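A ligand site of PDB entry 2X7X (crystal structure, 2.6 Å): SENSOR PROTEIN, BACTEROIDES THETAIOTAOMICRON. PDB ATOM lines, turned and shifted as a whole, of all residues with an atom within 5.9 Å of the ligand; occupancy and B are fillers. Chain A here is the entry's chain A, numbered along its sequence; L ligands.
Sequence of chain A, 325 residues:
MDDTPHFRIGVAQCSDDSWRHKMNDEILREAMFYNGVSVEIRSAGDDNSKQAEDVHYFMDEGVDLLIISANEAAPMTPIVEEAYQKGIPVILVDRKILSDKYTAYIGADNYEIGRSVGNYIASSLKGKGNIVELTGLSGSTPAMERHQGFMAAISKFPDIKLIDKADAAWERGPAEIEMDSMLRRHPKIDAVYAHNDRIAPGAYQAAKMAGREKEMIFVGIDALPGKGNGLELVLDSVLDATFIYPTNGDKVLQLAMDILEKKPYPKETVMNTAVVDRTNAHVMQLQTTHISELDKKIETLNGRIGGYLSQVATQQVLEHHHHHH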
ATOM      1  N   CYS A  14      -2.830   3.707 -14.403  1.00  0.00           N
ATOM      2  CA  CYS A  14      -2.140   2.505 -13.947  1.00  0.00           C
ATOM      3  C   CYS A  14      -2.541   1.232 -14.691  1.00  0.00           C
ATOM      4  O   CYS A  14      -1.774   0.271 -14.767  1.00  0.00           O
ATOM      5  CB  CYS A  14      -2.321   2.311 -12.430  1.00  0.00           C
ATOM      6  SG  CYS A  14      -4.048   2.253 -11.853  1.00  0.00           S
ATOM      7  N   SER A  15      -3.737   1.232 -15.242  1.00  0.00           N
ATOM      8  CA  SER A  15      -4.207   0.057 -15.956  1.00  0.00           C
ATOM      9  C   SER A  15      -5.332   0.402 -16.918  1.00  0.00           C
ATOM     10  O   SER A  15      -5.709   1.565 -17.047  1.00  0.00           O
ATOM     11  CB  SER A  15      -4.650  -1.047 -14.983  1.00  0.00           C
ATOM     12  OG  SER A  15      -5.395  -0.535 -13.905  1.00  0.00           O
ATOM     13  N   ASP A  16      -5.857  -0.633 -17.577  1.00  0.00           N
ATOM     14  CA  ASP A  16      -6.926  -0.477 -18.568  1.00  0.00           C
ATOM     15  C   ASP A  16      -8.002  -1.560 -18.457  1.00  0.00           C
ATOM     16  O   ASP A  16      -7.710  -2.738 -18.570  1.00  0.00           O
ATOM     17  CB  ASP A  16      -6.340  -0.493 -19.979  1.00  0.00           C
ATOM     18  CG  ASP A  16      -7.414  -0.438 -21.033  1.00  0.00           C
ATOM     19  OD1 ASP A  16      -8.120   0.604 -21.107  1.00  0.00           O
ATOM     20  OD2 ASP A  16      -7.569  -1.466 -21.754  1.00  0.00           O
ATOM     21  N   ASP A  17      -9.249  -1.122 -18.247  1.00  0.00           N
ATOM     22  CA  ASP A  17     -10.409  -1.989 -17.999  1.00  0.00           C
ATOM     23  C   ASP A  17     -11.685  -1.139 -18.072  1.00  0.00           C
ATOM     24  O   ASP A  17     -11.606   0.064 -18.316  1.00  0.00           O
ATOM     25  CB  ASP A  17     -10.304  -2.650 -16.618  1.00  0.00           C
ATOM     26  CG  ASP A  17      -9.892  -1.665 -15.524  1.00  0.00           C
ATOM     27  OD1 ASP A  17      -8.870  -1.942 -14.846  1.00  0.00           O
ATOM     28  OD2 ASP A  17     -10.555  -0.613 -15.337  1.00  0.00           O
ATOM     29  N   TRP A  19     -13.593   0.052 -15.812  1.00  0.00           N
ATOM     30  CA  TRP A  19     -13.603   1.124 -14.813  1.00  0.00           C
ATOM     31  C   TRP A  19     -12.799   2.337 -15.308  1.00  0.00           C
ATOM     32  O   TRP A  19     -13.324   3.443 -15.363  1.00  0.00           O
ATOM     33  CB  TRP A  19     -13.090   0.620 -13.466  1.00  0.00           C
ATOM     34  CG  TRP A  19     -13.319   1.584 -12.347  1.00  0.00           C
ATOM     35  CD1 TRP A  19     -14.396   1.627 -11.513  1.00  0.00           C
ATOM     36  CD2 TRP A  19     -12.458   2.666 -11.958  1.00  0.00           C
ATOM     37  NE1 TRP A  19     -14.256   2.667 -10.616  1.00  0.00           N
ATOM     38  CE2 TRP A  19     -13.082   3.312 -10.873  1.00  0.00           C
ATOM     39  CE3 TRP A  19     -11.224   3.144 -12.419  1.00  0.00           C
ATOM     40  CZ2 TRP A  19     -12.505   4.420 -10.240  1.00  0.00           C
ATOM     41  CZ3 TRP A  19     -10.660   4.235 -11.790  1.00  0.00           C
ATOM     42  CH2 TRP A  19     -11.298   4.864 -10.708  1.00  0.00           C
ATOM     43  N   ARG A  20     -11.545   2.112 -15.693  1.00  0.00           N
ATOM     44  CA  ARG A  20     -10.748   3.153 -16.355  1.00  0.00           C
ATOM     45  C   ARG A  20     -11.440   3.694 -17.620  1.00  0.00           C
ATOM     46  O   ARG A  20     -11.547   4.916 -17.806  1.00  0.00           O
ATOM     47  CB  ARG A  20      -9.323   2.670 -16.689  1.00  0.00           C
ATOM     48  CG  ARG A  20      -8.563   2.035 -15.532  1.00  0.00           C
ATOM     49  CD  ARG A  20      -8.116   3.031 -14.459  1.00  0.00           C
ATOM     50  NE  ARG A  20      -7.795   2.368 -13.198  1.00  0.00           N
ATOM     51  CZ  ARG A  20      -7.470   2.999 -12.065  1.00  0.00           C
ATOM     52  NH1 ARG A  20      -7.206   2.300 -10.966  1.00  0.00           N
ATOM     53  NH2 ARG A  20      -7.381   4.334 -12.020  1.00  0.00           N
ATOM     54  N   SER A  69      -2.831   8.135 -11.751  1.00  0.00           N
ATOM     55  CA  SER A  69      -3.247   7.159 -10.767  1.00  0.00           C
ATOM     56  C   SER A  69      -2.092   6.187 -10.500  1.00  0.00           C
ATOM     57  O   SER A  69      -1.828   5.282 -11.309  1.00  0.00           O
ATOM     58  CB  SER A  69      -4.505   6.426 -11.250  1.00  0.00           C
ATOM     59  OG  SER A  69      -4.643   5.178 -10.582  1.00  0.00           O
ATOM     60  N   ASP A  94      -7.613   8.636  -7.290  1.00  0.00           N
ATOM     61  CA  ASP A  94      -7.934   7.254  -6.889  1.00  0.00           C
ATOM     62  C   ASP A  94      -6.806   6.589  -6.069  1.00  0.00           C
ATOM     63  O   ASP A  94      -6.983   6.333  -4.885  1.00  0.00           O
ATOM     64  CB  ASP A  94      -8.420   6.429  -8.120  1.00  0.00           C
ATOM     65  CG  ASP A  94      -8.020   4.969  -8.069  1.00  0.00           C
ATOM     66  OD1 ASP A  94      -8.350   4.273  -7.083  1.00  0.00           O
ATOM     67  OD2 ASP A  94      -7.397   4.494  -9.034  1.00  0.00           O
ATOM     68  N   ARG A  95      -5.666   6.320  -6.690  1.00  0.00           N
ATOM     69  CA  ARG A  95      -4.519   5.804  -5.951  1.00  0.00           C
ATOM     70  C   ARG A  95      -3.600   6.936  -5.527  1.00  0.00           C
ATOM     71  O   ARG A  95      -3.583   7.978  -6.161  1.00  0.00           O
ATOM     72  CB  ARG A  95      -3.760   4.786  -6.775  1.00  0.00           C
ATOM     73  CG  ARG A  95      -4.669   3.741  -7.321  1.00  0.00           C
ATOM     74  CD  ARG A  95      -3.927   2.499  -7.731  1.00  0.00           C
ATOM     75  NE  ARG A  95      -4.872   1.564  -8.322  1.00  0.00           N
ATOM     76  CZ  ARG A  95      -4.533   0.452  -8.969  1.00  0.00           C
ATOM     77  NH1 ARG A  95      -3.257   0.116  -9.135  1.00  0.00           N
ATOM     78  NH2 ARG A  95      -5.488  -0.289  -9.465  1.00  0.00           N
ATOM     79  N   ASN A 110     -10.947   4.858   0.553  1.00  0.00           N
ATOM     80  CA  ASN A 110     -10.870   3.408   0.484  1.00  0.00           C
ATOM     81  C   ASN A 110     -10.939   2.736   1.842  1.00  0.00           C
ATOM     82  O   ASN A 110     -11.404   1.606   1.948  1.00  0.00           O
ATOM     83  CB  ASN A 110      -9.661   2.961  -0.351  1.00  0.00           C
ATOM     84  CG  ASN A 110      -9.895   3.154  -1.854  1.00  0.00           C
ATOM     85  OD1 ASN A 110     -10.589   2.372  -2.487  1.00  0.00           O
ATOM     86  ND2 ASN A 110      -9.347   4.219  -2.403  1.00  0.00           N
ATOM     87  N   PRO A 142      -5.309   1.655  -2.639  1.00  0.00           N
ATOM     88  CA  PRO A 142      -6.641   1.140  -2.346  1.00  0.00           C
ATOM     89  C   PRO A 142      -6.610  -0.262  -1.726  1.00  0.00           C
ATOM     90  O   PRO A 142      -7.324  -0.493  -0.760  1.00  0.00           O
ATOM     91  CB  PRO A 142      -7.352   1.180  -3.698  1.00  0.00           C
ATOM     92  CG  PRO A 142      -6.623   2.242  -4.446  1.00  0.00           C
ATOM     93  CD  PRO A 142      -5.200   2.079  -4.046  1.00  0.00           C
ATOM     94  N   ARG A 146      -8.451  -0.723   1.708  1.00  0.00           N
ATOM     95  CA  ARG A 146      -9.533  -1.702   1.704  1.00  0.00           C
ATOM     96  C   ARG A 146      -9.322  -2.824   2.729  1.00  0.00           C
ATOM     97  O   ARG A 146     -10.284  -3.348   3.285  1.00  0.00           O
ATOM     98  CB  ARG A 146      -9.786  -2.259   0.297  1.00  0.00           C
ATOM     99  CG  ARG A 146     -10.599  -1.299  -0.546  1.00  0.00           C
ATOM    100  CD  ARG A 146     -10.485  -1.563  -2.028  1.00  0.00           C
ATOM    101  NE  ARG A 146     -10.891  -0.390  -2.796  1.00  0.00           N
ATOM    102  CZ  ARG A 146     -11.147  -0.371  -4.110  1.00  0.00           C
ATOM    103  NH1 ARG A 146     -11.066  -1.489  -4.831  1.00  0.00           N
ATOM    104  NH2 ARG A 146     -11.468   0.783  -4.699  1.00  0.00           N
ATOM    105  N   TRP A 170      -6.080  -7.260  -8.493  1.00  0.00           N
ATOM    106  CA  TRP A 170      -7.242  -6.599  -9.104  1.00  0.00           C
ATOM    107  C   TRP A 170      -7.966  -7.420 -10.167  1.00  0.00           C
ATOM    108  O   TRP A 170      -8.885  -6.932 -10.801  1.00  0.00           O
ATOM    109  CB  TRP A 170      -6.875  -5.230  -9.684  1.00  0.00           C
ATOM    110  CG  TRP A 170      -6.340  -4.274  -8.660  1.00  0.00           C
ATOM    111  CD1 TRP A 170      -5.084  -3.742  -8.613  1.00  0.00           C
ATOM    112  CD2 TRP A 170      -7.044  -3.719  -7.523  1.00  0.00           C
ATOM    113  NE1 TRP A 170      -4.955  -2.901  -7.540  1.00  0.00           N
ATOM    114  CE2 TRP A 170      -6.136  -2.871  -6.845  1.00  0.00           C
ATOM    115  CE3 TRP A 170      -8.352  -3.867  -7.026  1.00  0.00           C
ATOM    116  CZ2 TRP A 170      -6.500  -2.169  -5.681  1.00  0.00           C
ATOM    117  CZ3 TRP A 170      -8.710  -3.163  -5.869  1.00  0.00           C
ATOM    118  CH2 TRP A 170      -7.777  -2.314  -5.211  1.00  0.00           C
ATOM    119  N   GLU A 171      -7.569  -8.673 -10.367  1.00  0.00           N
ATOM    120  CA  GLU A 171      -8.037  -9.371 -11.543  1.00  0.00           C
ATOM    121  C   GLU A 171      -8.706 -10.683 -11.249  1.00  0.00           C
ATOM    122  O   GLU A 171      -8.462 -11.282 -10.213  1.00  0.00           O
ATOM    123  CB  GLU A 171      -6.904  -9.541 -12.558  1.00  0.00           C
ATOM    124  CG  GLU A 171      -6.304  -8.248 -13.136  1.00  0.00           C
ATOM    125  CD  GLU A 171      -7.323  -7.214 -13.565  1.00  0.00           C
ATOM    126  OE1 GLU A 171      -7.069  -6.017 -13.317  1.00  0.00           O
ATOM    127  OE2 GLU A 171      -8.364  -7.561 -14.172  1.00  0.00           O
ATOM    128  N   HIS A 195     -11.783  -7.296  -3.435  1.00  0.00           N
ATOM    129  CA  HIS A 195     -11.463  -5.856  -3.516  1.00  0.00           C
ATOM    130  C   HIS A 195     -12.027  -5.166  -4.762  1.00  0.00           C
ATOM    131  O   HIS A 195     -12.145  -3.951  -4.789  1.00  0.00           O
ATOM    132  CB  HIS A 195      -9.948  -5.597  -3.392  1.00  0.00           C
ATOM    133  CG  HIS A 195      -9.427  -5.686  -1.983  1.00  0.00           C
ATOM    134  ND1 HIS A 195      -8.247  -5.086  -1.592  1.00  0.00           N
ATOM    135  CD2 HIS A 195      -9.934  -6.276  -0.879  1.00  0.00           C
ATOM    136  CE1 HIS A 195      -8.036  -5.322  -0.304  1.00  0.00           C
ATOM    137  NE2 HIS A 195      -9.049  -6.051   0.144  1.00  0.00           N
ATOM    138  N   ASN A 196     -12.374  -5.936  -5.788  1.00  0.00           N
ATOM    139  CA  ASN A 196     -13.184  -5.355  -6.856  1.00  0.00           C
ATOM    140  C   ASN A 196     -14.145  -6.337  -7.501  1.00  0.00           C
ATOM    141  O   ASN A 196     -14.142  -7.527  -7.190  1.00  0.00           O
ATOM    142  CB  ASN A 196     -12.339  -4.608  -7.906  1.00  0.00           C
ATOM    143  CG  ASN A 196     -11.570  -5.539  -8.851  1.00  0.00           C
ATOM    144  OD1 ASN A 196     -11.611  -6.783  -8.762  1.00  0.00           O
ATOM    145  ND2 ASN A 196     -10.869  -4.919  -9.792  1.00  0.00           N
ATOM    146  N   ASP A 197     -14.961  -5.810  -8.422  1.00  0.00           N
ATOM    147  CA  ASP A 197     -16.002  -6.574  -9.113  1.00  0.00           C
ATOM    148  C   ASP A 197     -15.441  -7.393 -10.251  1.00  0.00           C
ATOM    149  O   ASP A 197     -16.216  -7.939 -11.042  1.00  0.00           O
ATOM    150  CB  ASP A 197     -17.070  -5.631  -9.675  1.00  0.00           C
ATOM    151  CG  ASP A 197     -17.830  -4.888  -8.600  1.00  0.00           C
ATOM    152  OD1 ASP A 197     -17.862  -5.339  -7.431  1.00  0.00           O
ATOM    153  OD2 ASP A 197     -18.416  -3.847  -8.922  1.00  0.00           O
ATOM    154  N   ARG A 198     -14.115  -7.454 -10.381  1.00  0.00           N
ATOM    155  CA  ARG A 198     -13.489  -8.379 -11.318  1.00  0.00           C
ATOM    156  C   ARG A 198     -12.925  -9.578 -10.540  1.00  0.00           C
ATOM    157  O   ARG A 198     -13.041 -10.740 -10.971  1.00  0.00           O
ATOM    158  CB  ARG A 198     -12.398  -7.692 -12.127  1.00  0.00           C
ATOM    159  CG  ARG A 198     -12.926  -6.664 -13.157  1.00  0.00           C
ATOM    160  CD  ARG A 198     -11.826  -6.167 -14.138  1.00  0.00           C
ATOM    161  NE  ARG A 198     -10.582  -5.700 -13.477  1.00  0.00           N
ATOM    162  CZ  ARG A 198     -10.446  -4.537 -12.846  1.00  0.00           C
ATOM    163  NH1 ARG A 198     -11.477  -3.687 -12.739  1.00  0.00           N
ATOM    164  NH2 ARG A 198      -9.287  -4.231 -12.291  1.00  0.00           N
ATOM    165  N   ILE A 221     -16.262  -4.478  -4.846  1.00  0.00           N
ATOM    166  CA  ILE A 221     -16.216  -3.018  -4.861  1.00  0.00           C
ATOM    167  C   ILE A 221     -16.168  -2.562  -6.319  1.00  0.00           C
ATOM    168  O   ILE A 221     -15.549  -3.229  -7.139  1.00  0.00           O
ATOM    169  CB  ILE A 221     -14.997  -2.472  -4.088  1.00  0.00           C
ATOM    170  CG1 ILE A 221     -15.032  -2.932  -2.634  1.00  0.00           C
ATOM    171  CG2 ILE A 221     -14.981  -0.943  -4.117  1.00  0.00           C
ATOM    172  CD1 ILE A 221     -13.727  -2.753  -1.874  1.00  0.00           C
ATOM    173  N   ASP A 222     -16.853  -1.452  -6.604  1.00  0.00           N
ATOM    174  CA  ASP A 222     -16.775  -0.711  -7.880  1.00  0.00           C
ATOM    175  C   ASP A 222     -18.172  -0.313  -8.301  1.00  0.00           C
ATOM    176  O   ASP A 222     -18.447   0.879  -8.525  1.00  0.00           O
ATOM    177  CB  ASP A 222     -16.071  -1.480  -9.007  1.00  0.00           C
ATOM    178  CG  ASP A 222     -14.553  -1.353  -8.964  1.00  0.00           C
ATOM    179  OD1 ASP A 222     -13.998  -0.443  -8.307  1.00  0.00           O
ATOM    180  OD2 ASP A 222     -13.886  -2.186  -9.602  1.00  0.00           O
ATOM    181  N   TYR A 245     -17.497   2.601  -6.266  1.00  0.00           N
ATOM    182  CA  TYR A 245     -16.206   3.268  -6.331  1.00  0.00           C
ATOM    183  C   TYR A 245     -16.253   4.217  -7.519  1.00  0.00           C
ATOM    184  O   TYR A 245     -16.063   3.799  -8.676  1.00  0.00           O
ATOM    185  CB  TYR A 245     -15.050   2.281  -6.423  1.00  0.00           C
ATOM    186  CG  TYR A 245     -13.705   2.937  -6.173  1.00  0.00           C
ATOM    187  CD1 TYR A 245     -13.453   3.607  -4.966  1.00  0.00           C
ATOM    188  CD2 TYR A 245     -12.694   2.885  -7.127  1.00  0.00           C
ATOM    189  CE1 TYR A 245     -12.219   4.226  -4.710  1.00  0.00           C
ATOM    190  CE2 TYR A 245     -11.456   3.485  -6.887  1.00  0.00           C
ATOM    191  CZ  TYR A 245     -11.233   4.155  -5.677  1.00  0.00           C
ATOM    192  OH  TYR A 245     -10.008   4.755  -5.409  1.00  0.00           O
HETATM  193  C1  LIG L   1      -9.713  -0.105 -11.902  1.00  0.00           C
HETATM  194  C2  LIG L   1      -9.550  -0.779 -10.546  1.00  0.00           C
HETATM  195  C3  LIG L   1     -10.882  -0.926  -9.818  1.00  0.00           C
HETATM  196  C4  LIG L   1     -10.495  -0.645  -8.380  1.00  0.00           C
HETATM  197  C5  LIG L   1      -9.478   0.475  -8.567  1.00  0.00           C
HETATM  198  C6  LIG L   1      -8.488   0.658  -7.423  1.00  0.00           C
HETATM  199  O1  LIG L   1      -8.537  -0.312 -12.684  1.00  0.00           O
HETATM  200  O2  LIG L   1      -8.893  -2.035 -10.751  1.00  0.00           O
HETATM  201  O3  LIG L   1     -11.488  -2.212 -10.018  1.00  0.00           O
HETATM  202  O4  LIG L   1     -11.606  -0.270  -7.558  1.00  0.00           O
HETATM  203  O5  LIG L   1      -8.746   0.061  -9.729  1.00  0.00           O
HETATM  204  O6  LIG L   1      -7.671   1.826  -7.672  1.00  0.00           O
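OD2 of Asp 222 is in hydrogen-bond range of O3 of the ligand, 2.4 Å away. The side-chain carboxylate of Asp 94 sits at hydrogen-bond distance from an oxygen (O6) of the ligand (2.6 Å). An oxygen (O2) of the ligand sits at hydrogen-bond distance from the guanidinium group (NH2) of Arg 198, at 2.7 Å. The side-chain carboxylate (OD1) of Asp 17 is in hydrogen-bond range of an oxygen (O1) of the ligand. O3 of the ligand is in hydrogen-bond range of ND2 of Asn 196 (2.8 Å). O1 of the ligand is in hydrogen-bond range of NE of Arg 20 (2.8 Å). NE of Arg 95 is in hydrogen-bond range of O6 of the ligand. The guanidinium group of Arg 146 is in hydrogen-bond range of an oxygen (O4) of the ligand, at 3.0 Å. An oxygen (O1) of the ligand is in hydrogen-bond range of the side-chain hydroxyl (OG) of Ser 15 (3.4 Å).
N of Tyr 245 lies within hydrogen-bond range of O of Asp 222. The guanidinium group of Arg 95 is in salt-bridge range of the side-chain carboxylate of Asp 94 (3.9 Å). The side-chain carboxylate of Asp 94 is in hydrogen-bond range of the side-chain hydroxyl of Tyr 245 (2.4 Å). The side-chain carboxylate (OD2) of Asp 94 is in hydrogen-bond range of the side-chain hydroxyl (OG) of Ser 69, 3.2 Å away. O of Trp 170 sits at hydrogen-bond distance from NH2 of Arg 198, at 3.1 Å. N of Trp 19 is in hydrogen-bond range of OD2 of Asp 17 (3.1 Å). The guanidinium group (NH1) of Arg 146 is in hydrogen-bond range of the backbone carbonyl oxygen (O) of His 195, at 2.7 Å. The side-chain amide nitrogen of Asn 110 lies within hydrogen-bond range of the side-chain hydroxyl of Tyr 245 (3.1 Å).
Trp 19 touches the ligand (CE3 to C1, 3.6 Å). Pro 142 touches the ligand. Trp 170 touches the ligand. CD2 of Tyr 245 touches O4 of the ligand, at 3.4 Å. Hydrophobic or aromatic side chains within 4 Å of the ligand: Trp 19, Pro 142, Trp 170 and Tyr 245. 13 residues have an atom within 4 Å of the ligand: Ser 15, Asp 17, Trp 19, Arg 20, Asp 94, Arg 95, Pro 142, Arg 146, Trp 170, Asn 196, Arg 198, Asp 222 and Tyr 245.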
